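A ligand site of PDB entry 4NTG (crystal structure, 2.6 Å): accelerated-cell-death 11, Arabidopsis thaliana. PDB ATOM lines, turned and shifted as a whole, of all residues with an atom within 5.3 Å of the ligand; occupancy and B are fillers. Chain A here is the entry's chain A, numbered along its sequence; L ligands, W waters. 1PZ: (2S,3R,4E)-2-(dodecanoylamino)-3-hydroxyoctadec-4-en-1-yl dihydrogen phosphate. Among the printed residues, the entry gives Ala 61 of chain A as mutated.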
ATOM      1  N   PHE A  48      -8.830  21.727  -6.537  1.00  0.00           N
ATOM      2  CA  PHE A  48      -8.145  22.967  -6.233  1.00  0.00           C
ATOM      3  C   PHE A  48      -9.129  24.130  -6.047  1.00  0.00           C
ATOM      4  O   PHE A  48      -8.886  25.019  -5.236  1.00  0.00           O
ATOM      5  CB  PHE A  48      -7.126  23.294  -7.316  1.00  0.00           C
ATOM      6  CG  PHE A  48      -6.025  22.273  -7.447  1.00  0.00           C
ATOM      7  CD1 PHE A  48      -5.107  22.090  -6.428  1.00  0.00           C
ATOM      8  CD2 PHE A  48      -5.897  21.498  -8.601  1.00  0.00           C
ATOM      9  CE1 PHE A  48      -4.071  21.148  -6.552  1.00  0.00           C
ATOM     10  CE2 PHE A  48      -4.878  20.571  -8.737  1.00  0.00           C
ATOM     11  CZ  PHE A  48      -3.967  20.393  -7.717  1.00  0.00           C
ATOM     12  N   LEU A  51     -10.691  24.405  -2.485  1.00  0.00           N
ATOM     13  CA  LEU A  51      -9.792  24.762  -1.391  1.00  0.00           C
ATOM     14  C   LEU A  51      -9.801  26.266  -1.073  1.00  0.00           C
ATOM     15  O   LEU A  51      -8.888  26.766  -0.411  1.00  0.00           O
ATOM     16  CB  LEU A  51      -8.381  24.252  -1.661  1.00  0.00           C
ATOM     17  CG  LEU A  51      -8.239  22.742  -1.898  1.00  0.00           C
ATOM     18  CD1 LEU A  51      -6.780  22.347  -2.078  1.00  0.00           C
ATOM     19  CD2 LEU A  51      -8.840  21.959  -0.754  1.00  0.00           C
ATOM     20  N   ALA A  54      -8.752  31.950  -2.686  1.00  0.00           N
ATOM     21  CA  ALA A  54      -7.361  32.200  -3.002  1.00  0.00           C
ATOM     22  C   ALA A  54      -6.824  31.088  -3.904  1.00  0.00           C
ATOM     23  O   ALA A  54      -6.085  31.341  -4.858  1.00  0.00           O
ATOM     24  CB  ALA A  54      -6.541  32.339  -1.724  1.00  0.00           C
ATOM     25  N   PHE A  55      -7.217  29.846  -3.608  1.00  0.00           N
ATOM     26  CA  PHE A  55      -6.722  28.686  -4.355  1.00  0.00           C
ATOM     27  C   PHE A  55      -7.399  28.432  -5.711  1.00  0.00           C
ATOM     28  O   PHE A  55      -7.037  27.490  -6.424  1.00  0.00           O
ATOM     29  CB  PHE A  55      -6.736  27.439  -3.465  1.00  0.00           C
ATOM     30  CG  PHE A  55      -5.616  27.440  -2.467  1.00  0.00           C
ATOM     31  CD1 PHE A  55      -4.332  27.829  -2.858  1.00  0.00           C
ATOM     32  CD2 PHE A  55      -5.842  27.115  -1.139  1.00  0.00           C
ATOM     33  CE1 PHE A  55      -3.281  27.870  -1.955  1.00  0.00           C
ATOM     34  CE2 PHE A  55      -4.781  27.135  -0.219  1.00  0.00           C
ATOM     35  CZ  PHE A  55      -3.509  27.511  -0.634  1.00  0.00           C
ATOM     36  N   PHE A  57      -6.882  30.470  -7.956  1.00  0.00           N
ATOM     37  CA  PHE A  57      -5.714  30.843  -8.758  1.00  0.00           C
ATOM     38  C   PHE A  57      -4.766  29.616  -8.943  1.00  0.00           C
ATOM     39  O   PHE A  57      -4.215  29.399 -10.035  1.00  0.00           O
ATOM     40  CB  PHE A  57      -4.971  32.042  -8.158  1.00  0.00           C
ATOM     41  CG  PHE A  57      -5.840  33.294  -8.001  1.00  0.00           C
ATOM     42  CD1 PHE A  57      -7.114  33.383  -8.573  1.00  0.00           C
ATOM     43  CD2 PHE A  57      -5.365  34.384  -7.272  1.00  0.00           C
ATOM     44  CE1 PHE A  57      -7.902  34.528  -8.429  1.00  0.00           C
ATOM     45  CE2 PHE A  57      -6.149  35.534  -7.120  1.00  0.00           C
ATOM     46  CZ  PHE A  57      -7.424  35.605  -7.695  1.00  0.00           C
ATOM     47  N   ALA A  58      -4.585  28.828  -7.888  1.00  0.00           N
ATOM     48  CA  ALA A  58      -3.856  27.568  -8.007  1.00  0.00           C
ATOM     49  C   ALA A  58      -4.556  26.626  -9.000  1.00  0.00           C
ATOM     50  O   ALA A  58      -3.897  25.898  -9.762  1.00  0.00           O
ATOM     51  CB  ALA A  58      -3.691  26.886  -6.641  1.00  0.00           C
ATOM     52  N   ALA A  61      -3.757  27.807 -12.585  1.00  0.00           N
ATOM     53  CA  ALA A  61      -2.382  27.476 -12.913  1.00  0.00           C
ATOM     54  C   ALA A  61      -2.272  26.004 -13.323  1.00  0.00           C
ATOM     55  O   ALA A  61      -1.513  25.664 -14.240  1.00  0.00           O
ATOM     56  CB  ALA A  61      -1.480  27.759 -11.747  1.00  0.00           C
ATOM     57  N   TYR A  62      -3.023  25.154 -12.645  1.00  0.00           N
ATOM     58  CA  TYR A  62      -3.080  23.730 -12.969  1.00  0.00           C
ATOM     59  C   TYR A  62      -3.843  23.502 -14.258  1.00  0.00           C
ATOM     60  O   TYR A  62      -3.348  22.781 -15.159  1.00  0.00           O
ATOM     61  CB  TYR A  62      -3.714  22.920 -11.832  1.00  0.00           C
ATOM     62  CG  TYR A  62      -3.824  21.434 -12.099  1.00  0.00           C
ATOM     63  CD1 TYR A  62      -2.704  20.609 -12.067  1.00  0.00           C
ATOM     64  CD2 TYR A  62      -5.054  20.851 -12.375  1.00  0.00           C
ATOM     65  CE1 TYR A  62      -2.812  19.238 -12.317  1.00  0.00           C
ATOM     66  CE2 TYR A  62      -5.174  19.482 -12.632  1.00  0.00           C
ATOM     67  CZ  TYR A  62      -4.052  18.691 -12.593  1.00  0.00           C
ATOM     68  OH  TYR A  62      -4.172  17.335 -12.833  1.00  0.00           O
ATOM     69  N   LYS A  65      -1.996  24.119 -17.570  1.00  0.00           N
ATOM     70  CA  LYS A  65      -1.081  23.054 -17.990  1.00  0.00           C
ATOM     71  C   LYS A  65      -1.840  21.873 -18.615  1.00  0.00           C
ATOM     72  O   LYS A  65      -1.478  21.389 -19.688  1.00  0.00           O
ATOM     73  CB  LYS A  65      -0.245  22.569 -16.804  1.00  0.00           C
ATOM     74  CG  LYS A  65       0.589  23.641 -16.127  1.00  0.00           C
ATOM     75  CD  LYS A  65       1.459  24.373 -17.137  1.00  0.00           C
ATOM     76  CE  LYS A  65       2.356  25.391 -16.440  1.00  0.00           C
ATOM     77  NZ  LYS A  65       2.743  26.454 -17.380  1.00  0.00           N
ATOM     78  N   ALA A  95       9.775  26.970 -21.884  1.00  0.00           N
ATOM     79  CA  ALA A  95       8.486  27.316 -21.276  1.00  0.00           C
ATOM     80  C   ALA A  95       7.370  27.074 -22.280  1.00  0.00           C
ATOM     81  O   ALA A  95       7.468  27.532 -23.425  1.00  0.00           O
ATOM     82  CB  ALA A  95       8.463  28.764 -20.825  1.00  0.00           C
ATOM     83  N   GLY A  96       6.334  26.346 -21.873  1.00  0.00           N
ATOM     84  CA  GLY A  96       5.223  26.058 -22.771  1.00  0.00           C
ATOM     85  C   GLY A  96       5.316  24.763 -23.578  1.00  0.00           C
ATOM     86  O   GLY A  96       4.373  24.397 -24.278  1.00  0.00           O
ATOM     87  N   ARG A 100       7.448  19.946 -20.639  1.00  0.00           N
ATOM     88  CA  ARG A 100       7.573  20.801 -19.469  1.00  0.00           C
ATOM     89  C   ARG A 100       6.246  20.855 -18.699  1.00  0.00           C
ATOM     90  O   ARG A 100       6.220  20.643 -17.479  1.00  0.00           O
ATOM     91  CB  ARG A 100       8.069  22.207 -19.837  1.00  0.00           C
ATOM     92  CG  ARG A 100       8.105  23.189 -18.636  1.00  0.00           C
ATOM     93  CD  ARG A 100       8.912  24.449 -18.968  1.00  0.00           C
ATOM     94  NE  ARG A 100       8.650  25.571 -18.064  1.00  0.00           N
ATOM     95  CZ  ARG A 100       9.467  26.610 -17.900  1.00  0.00           C
ATOM     96  NH1 ARG A 100      10.601  26.670 -18.580  1.00  0.00           N
ATOM     97  NH2 ARG A 100       9.138  27.590 -17.063  1.00  0.00           N
ATOM     98  N   ASN A 101       5.138  21.100 -19.407  1.00  0.00           N
ATOM     99  CA  ASN A 101       3.831  21.086 -18.772  1.00  0.00           C
ATOM    100  C   ASN A 101       3.501  19.727 -18.181  1.00  0.00           C
ATOM    101  O   ASN A 101       2.818  19.649 -17.146  1.00  0.00           O
ATOM    102  CB  ASN A 101       2.738  21.483 -19.759  1.00  0.00           C
ATOM    103  CG  ASN A 101       2.954  22.860 -20.350  1.00  0.00           C
ATOM    104  OD1 ASN A 101       3.495  23.768 -19.700  1.00  0.00           O
ATOM    105  ND2 ASN A 101       2.545  23.022 -21.606  1.00  0.00           N
ATOM    106  N   ARG A 104       4.893  19.570 -14.782  1.00  0.00           N
ATOM    107  CA  ARG A 104       4.126  20.333 -13.799  1.00  0.00           C
ATOM    108  C   ARG A 104       2.837  19.612 -13.426  1.00  0.00           C
ATOM    109  O   ARG A 104       2.452  19.569 -12.254  1.00  0.00           O
ATOM    110  CB  ARG A 104       3.860  21.767 -14.246  1.00  0.00           C
ATOM    111  CG  ARG A 104       5.067  22.685 -14.075  1.00  0.00           C
ATOM    112  CD  ARG A 104       5.875  22.805 -15.365  1.00  0.00           C
ATOM    113  NE  ARG A 104       6.974  23.756 -15.241  1.00  0.00           N
ATOM    114  CZ  ARG A 104       8.185  23.437 -14.769  1.00  0.00           C
ATOM    115  NH1 ARG A 104       9.140  24.354 -14.677  1.00  0.00           N
ATOM    116  NH2 ARG A 104       8.429  22.198 -14.369  1.00  0.00           N
ATOM    117  N   GLY A 108       1.093  18.243  -9.870  1.00  0.00           N
ATOM    118  CA  GLY A 108      -0.301  18.440  -9.490  1.00  0.00           C
ATOM    119  C   GLY A 108      -0.905  17.148  -8.964  1.00  0.00           C
ATOM    120  O   GLY A 108      -1.483  17.146  -7.860  1.00  0.00           O
ATOM    121  N   MET A 111       0.606  16.207  -5.681  1.00  0.00           N
ATOM    122  CA  MET A 111       0.003  17.141  -4.731  1.00  0.00           C
ATOM    123  C   MET A 111      -1.312  16.613  -4.145  1.00  0.00           C
ATOM    124  O   MET A 111      -1.456  16.498  -2.938  1.00  0.00           O
ATOM    125  CB  MET A 111      -0.280  18.491  -5.398  1.00  0.00           C
ATOM    126  CG  MET A 111      -1.011  19.479  -4.483  1.00  0.00           C
ATOM    127  SD  MET A 111       0.045  19.889  -3.078  1.00  0.00           S
ATOM    128  CE  MET A 111      -1.093  20.711  -1.984  1.00  0.00           C
ATOM    129  N   ALA A 132      -2.846  20.408   4.054  1.00  0.00           N
ATOM    130  CA  ALA A 132      -2.527  21.270   2.904  1.00  0.00           C
ATOM    131  C   ALA A 132      -1.079  21.805   2.909  1.00  0.00           C
ATOM    132  O   ALA A 132      -0.424  21.797   1.870  1.00  0.00           O
ATOM    133  CB  ALA A 132      -3.536  22.417   2.804  1.00  0.00           C
ATOM    134  N   TYR A 136       1.829  20.389   0.338  1.00  0.00           N
ATOM    135  CA  TYR A 136       2.444  21.403  -0.498  1.00  0.00           C
ATOM    136  C   TYR A 136       3.963  21.538  -0.235  1.00  0.00           C
ATOM    137  O   TYR A 136       4.755  21.693  -1.179  1.00  0.00           O
ATOM    138  CB  TYR A 136       1.760  22.760  -0.315  1.00  0.00           C
ATOM    139  CG  TYR A 136       2.357  23.810  -1.209  1.00  0.00           C
ATOM    140  CD1 TYR A 136       1.943  23.928  -2.539  1.00  0.00           C
ATOM    141  CD2 TYR A 136       3.352  24.667  -0.752  1.00  0.00           C
ATOM    142  CE1 TYR A 136       2.477  24.868  -3.370  1.00  0.00           C
ATOM    143  CE2 TYR A 136       3.907  25.618  -1.588  1.00  0.00           C
ATOM    144  CZ  TYR A 136       3.463  25.708  -2.889  1.00  0.00           C
ATOM    145  OH  TYR A 136       4.009  26.649  -3.727  1.00  0.00           O
ATOM    146  N   PHE A 140       5.688  20.674  -3.835  1.00  0.00           N
ATOM    147  CA  PHE A 140       6.042  21.876  -4.581  1.00  0.00           C
ATOM    148  C   PHE A 140       7.131  22.780  -3.975  1.00  0.00           C
ATOM    149  O   PHE A 140       7.691  23.633  -4.679  1.00  0.00           O
ATOM    150  CB  PHE A 140       4.795  22.711  -4.860  1.00  0.00           C
ATOM    151  CG  PHE A 140       3.930  22.188  -5.988  1.00  0.00           C
ATOM    152  CD1 PHE A 140       4.378  22.225  -7.312  1.00  0.00           C
ATOM    153  CD2 PHE A 140       2.650  21.698  -5.733  1.00  0.00           C
ATOM    154  CE1 PHE A 140       3.563  21.770  -8.352  1.00  0.00           C
ATOM    155  CE2 PHE A 140       1.823  21.239  -6.753  1.00  0.00           C
ATOM    156  CZ  PHE A 140       2.287  21.264  -8.079  1.00  0.00           C
ATOM    157  N   HIS A 144       8.622  25.492  -6.582  1.00  0.00           N
ATOM    158  CA  HIS A 144       8.089  26.853  -6.625  1.00  0.00           C
ATOM    159  C   HIS A 144       9.024  27.880  -5.976  1.00  0.00           C
ATOM    160  O   HIS A 144       9.571  27.633  -4.908  1.00  0.00           O
ATOM    161  CB  HIS A 144       6.704  26.920  -5.990  1.00  0.00           C
ATOM    162  CG  HIS A 144       5.638  26.245  -6.794  1.00  0.00           C
ATOM    163  ND1 HIS A 144       4.379  25.989  -6.310  1.00  0.00           N
ATOM    164  CD2 HIS A 144       5.656  25.777  -8.068  1.00  0.00           C
ATOM    165  CE1 HIS A 144       3.662  25.396  -7.246  1.00  0.00           C
ATOM    166  NE2 HIS A 144       4.417  25.261  -8.323  1.00  0.00           N
ATOM    167  N   ILE A 148       6.021  32.561  -5.318  1.00  0.00           N
ATOM    168  CA  ILE A 148       4.861  31.692  -5.428  1.00  0.00           C
ATOM    169  C   ILE A 148       4.514  31.073  -4.077  1.00  0.00           C
ATOM    170  O   ILE A 148       3.349  31.039  -3.689  1.00  0.00           O
ATOM    171  CB  ILE A 148       5.132  30.550  -6.437  1.00  0.00           C
ATOM    172  CG1 ILE A 148       5.418  31.099  -7.833  1.00  0.00           C
ATOM    173  CG2 ILE A 148       3.968  29.563  -6.462  1.00  0.00           C
ATOM    174  CD1 ILE A 148       4.214  31.673  -8.482  1.00  0.00           C
ATOM    175  N   ALA A 151       2.674  33.438  -1.708  1.00  0.00           N
ATOM    176  CA  ALA A 151       1.264  33.473  -2.135  1.00  0.00           C
ATOM    177  C   ALA A 151       0.493  32.249  -1.643  1.00  0.00           C
ATOM    178  O   ALA A 151      -0.601  32.393  -1.072  1.00  0.00           O
ATOM    179  CB  ALA A 151       1.175  33.570  -3.656  1.00  0.00           C
ATOM    180  N   VAL A 152       1.056  31.074  -1.878  1.00  0.00           N
ATOM    181  CA  VAL A 152       0.384  29.831  -1.489  1.00  0.00           C
ATOM    182  C   VAL A 152       0.200  29.825   0.029  1.00  0.00           C
ATOM    183  O   VAL A 152      -0.848  29.395   0.541  1.00  0.00           O
ATOM    184  CB  VAL A 152       1.161  28.599  -1.976  1.00  0.00           C
ATOM    185  CG1 VAL A 152       0.839  27.401  -1.113  1.00  0.00           C
ATOM    186  CG2 VAL A 152       0.831  28.299  -3.412  1.00  0.00           C
ATOM    187  N   LEU A 154      -0.154  32.337   1.962  1.00  0.00           N
ATOM    188  CA  LEU A 154      -1.268  33.235   2.234  1.00  0.00           C
ATOM    189  C   LEU A 154      -2.599  32.561   1.908  1.00  0.00           C
ATOM    190  O   LEU A 154      -3.591  32.745   2.628  1.00  0.00           O
ATOM    191  CB  LEU A 154      -1.090  34.502   1.410  1.00  0.00           C
ATOM    192  CG  LEU A 154      -2.295  35.430   1.383  1.00  0.00           C
ATOM    193  CD1 LEU A 154      -2.565  35.961   2.778  1.00  0.00           C
ATOM    194  CD2 LEU A 154      -2.036  36.562   0.425  1.00  0.00           C
ATOM    195  N   GLY A 155      -2.614  31.750   0.844  1.00  0.00           N
ATOM    196  CA  GLY A 155      -3.826  31.066   0.425  1.00  0.00           C
ATOM    197  C   GLY A 155      -4.371  30.151   1.507  1.00  0.00           C
ATOM    198  O   GLY A 155      -5.592  29.947   1.591  1.00  0.00           O
ATOM    199  N   MET A 156      -3.474  29.624   2.339  1.00  0.00           N
ATOM    200  CA  MET A 156      -3.867  28.726   3.421  1.00  0.00           C
ATOM    201  C   MET A 156      -4.906  29.360   4.348  1.00  0.00           C
ATOM    202  O   MET A 156      -5.727  28.648   4.945  1.00  0.00           O
ATOM    203  CB  MET A 156      -2.640  28.257   4.216  1.00  0.00           C
ATOM    204  CG  MET A 156      -1.648  27.445   3.389  1.00  0.00           C
ATOM    205  SD  MET A 156      -2.324  25.924   2.680  1.00  0.00           S
ATOM    206  CE  MET A 156      -0.848  25.318   1.836  1.00  0.00           C
HETATM  207  CAS 1PZ L   1      -4.489  37.686  -1.943  1.00  0.00           C
HETATM  208  CAF 1PZ L   1      -5.094  36.561  -2.784  1.00  0.00           C
HETATM  209  CAG 1PZ L   1      -4.409  35.242  -2.411  1.00  0.00           C
HETATM  210  CAH 1PZ L   1      -3.484  34.794  -3.555  1.00  0.00           C
HETATM  211  CAI 1PZ L   1      -2.741  33.495  -3.147  1.00  0.00           C
HETATM  212  CAJ 1PZ L   1      -2.224  32.780  -4.393  1.00  0.00           C
HETATM  213  CAK 1PZ L   1      -2.689  31.319  -4.332  1.00  0.00           C
HETATM  214  CAL 1PZ L   1      -1.552  30.414  -4.858  1.00  0.00           C
HETATM  215  CAM 1PZ L   1      -1.567  30.345  -6.396  1.00  0.00           C
HETATM  216  CAN 1PZ L   1      -0.630  29.151  -6.763  1.00  0.00           C
HETATM  217  CAO 1PZ L   1      -0.330  29.191  -8.271  1.00  0.00           C
HETATM  218  CAP 1PZ L   1       1.157  28.765  -8.450  1.00  0.00           C
HETATM  219  CAQ 1PZ L   1       1.254  27.772  -9.628  1.00  0.00           C
HETATM  220  CAE 1PZ L   1       2.632  27.907 -10.235  1.00  0.00           C
HETATM  221  CAD 1PZ L   1       2.776  28.417 -11.527  1.00  0.00           C
HETATM  222  CAC 1PZ L   1       4.116  28.245 -12.271  1.00  0.00           C
HETATM  223  OAR 1PZ L   1       5.129  28.865 -11.560  1.00  0.00           O
HETATM  224  CAB 1PZ L   1       4.385  26.761 -12.376  1.00  0.00           C
HETATM  225  CAA 1PZ L   1       5.360  26.509 -13.508  1.00  0.00           C
HETATM  226  OBB 1PZ L   1       4.757  26.717 -14.773  1.00  0.00           O
HETATM  227  PAX 1PZ L   1       5.656  27.223 -15.981  1.00  0.00           P
HETATM  228  OAZ 1PZ L   1       4.690  27.902 -16.878  1.00  0.00           O
HETATM  229  OBA 1PZ L   1       6.151  25.957 -16.786  1.00  0.00           O
HETATM  230  OAY 1PZ L   1       6.779  28.103 -15.553  1.00  0.00           O
HETATM  231  NAW 1PZ L   1       3.156  26.053 -12.591  1.00  0.00           N
HETATM  232  CAU 1PZ L   1       2.895  24.870 -11.925  1.00  0.00           C
HETATM  233  OAV 1PZ L   1       3.781  24.192 -11.161  1.00  0.00           O
HETATM  234  CAT 1PZ L   1       1.458  24.349 -12.115  1.00  0.00           C
HETATM  235  CBC 1PZ L   1       1.068  23.583 -10.817  1.00  0.00           C
HETATM  236  CBD 1PZ L   1      -0.391  23.850 -10.562  1.00  0.00           C
HETATM  237  CBE 1PZ L   1      -0.840  23.229  -9.207  1.00  0.00           C
HETATM  238  CBF 1PZ L   1      -0.034  23.868  -8.057  1.00  0.00           C
HETATM  239  CBG 1PZ L   1      -0.990  24.621  -7.096  1.00  0.00           C
HETATM  240  CBH 1PZ L   1      -1.394  23.666  -5.968  1.00  0.00           C
HETATM  241  CBI 1PZ L   1      -1.262  24.401  -4.620  1.00  0.00           C
HETATM  242  CBJ 1PZ L   1      -2.113  23.631  -3.625  1.00  0.00           C
HETATM  243  CBK 1PZ L   1      -2.266  24.432  -2.336  1.00  0.00           C
HETATM  244  CBL 1PZ L   1      -3.425  23.828  -1.560  1.00  0.00           C
HETATM  245  O   HOH W   1       6.980  30.709 -14.756  1.00  0.00           O
HETATM  246  O   HOH W   2       7.773  28.379 -10.485  1.00  0.00           O
HETATM  247  O   HOH W   3       6.372  23.213 -10.515  1.00  0.00           O
HETATM  248  O   HOH W   4       7.652  25.435 -11.401  1.00  0.00           O
HETATM  249  O   HOH W   5       8.372  26.659 -14.011  1.00  0.00           O
HETATM  250  O   HOH W   6       5.688  25.591 -19.323  1.00  0.00           O
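ND1 of His 144 lies within hydrogen-bond range of OH of Tyr 136, at 2.7 Å.
A ring nitrogen (NE2) of His 144 sits at hydrogen-bond distance from an oxygen (OAV) of the ligand, 3.1 Å away.
An oxygen (OBA) of the ligand is in salt-bridge range of the guanidinium group of Arg 100, at 2.8 Å.
NE of Arg 104 lies within salt-bridge range of OBA of the ligand (2.8 Å).
OAZ of the ligand is in salt-bridge range of NZ of Lys 65, at 2.5 Å.
Phe 48 touches the ligand.
Leu 51 touches the ligand (CD1 to CBL, 3.7 Å).
O of Ala 54 touches CAK of the ligand, 3.4 Å away.
CE1 of Phe 55 touches CBK of the ligand (3.6 Å).
CB of Ala 58 touches CBG of the ligand (3.6 Å).
Ala 61 touches the ligand.
Tyr 62 touches the ligand.
CE of Met 111 touches CBJ of the ligand, at 3.5 Å.
CD1 of Tyr 136 touches CBI of the ligand, at 3.9 Å.
Phe 140 touches the ligand (CE2 to CBF, 3.5 Å).
Ile 148 touches the ligand.
O of Ala 151 touches CAI of the ligand, at 3.2 Å.
CG2 of Val 152 touches CAL of the ligand, 3.5 Å away.
Leu 154 touches the ligand.
The nearest printed residue that does not touch the ligand is Phe 57 (4.2 Å).
Water W6 lies within hydrogen-bond range of an oxygen (OBA) of the ligand (2.6 Å), the backbone NH (N) of Gly 96 (2.7 Å), the side-chain amide oxygen (OD1) of Asn 101 (2.9 Å) and the guanidinium group (NE) of Arg 100 (3.2 Å).
Water W5 lies within hydrogen-bond range of the guanidinium group of Arg 104 (2.5 Å), an oxygen (OAY) of the ligand (2.6 Å) and the guanidinium group of Arg 100 (3.3 Å).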
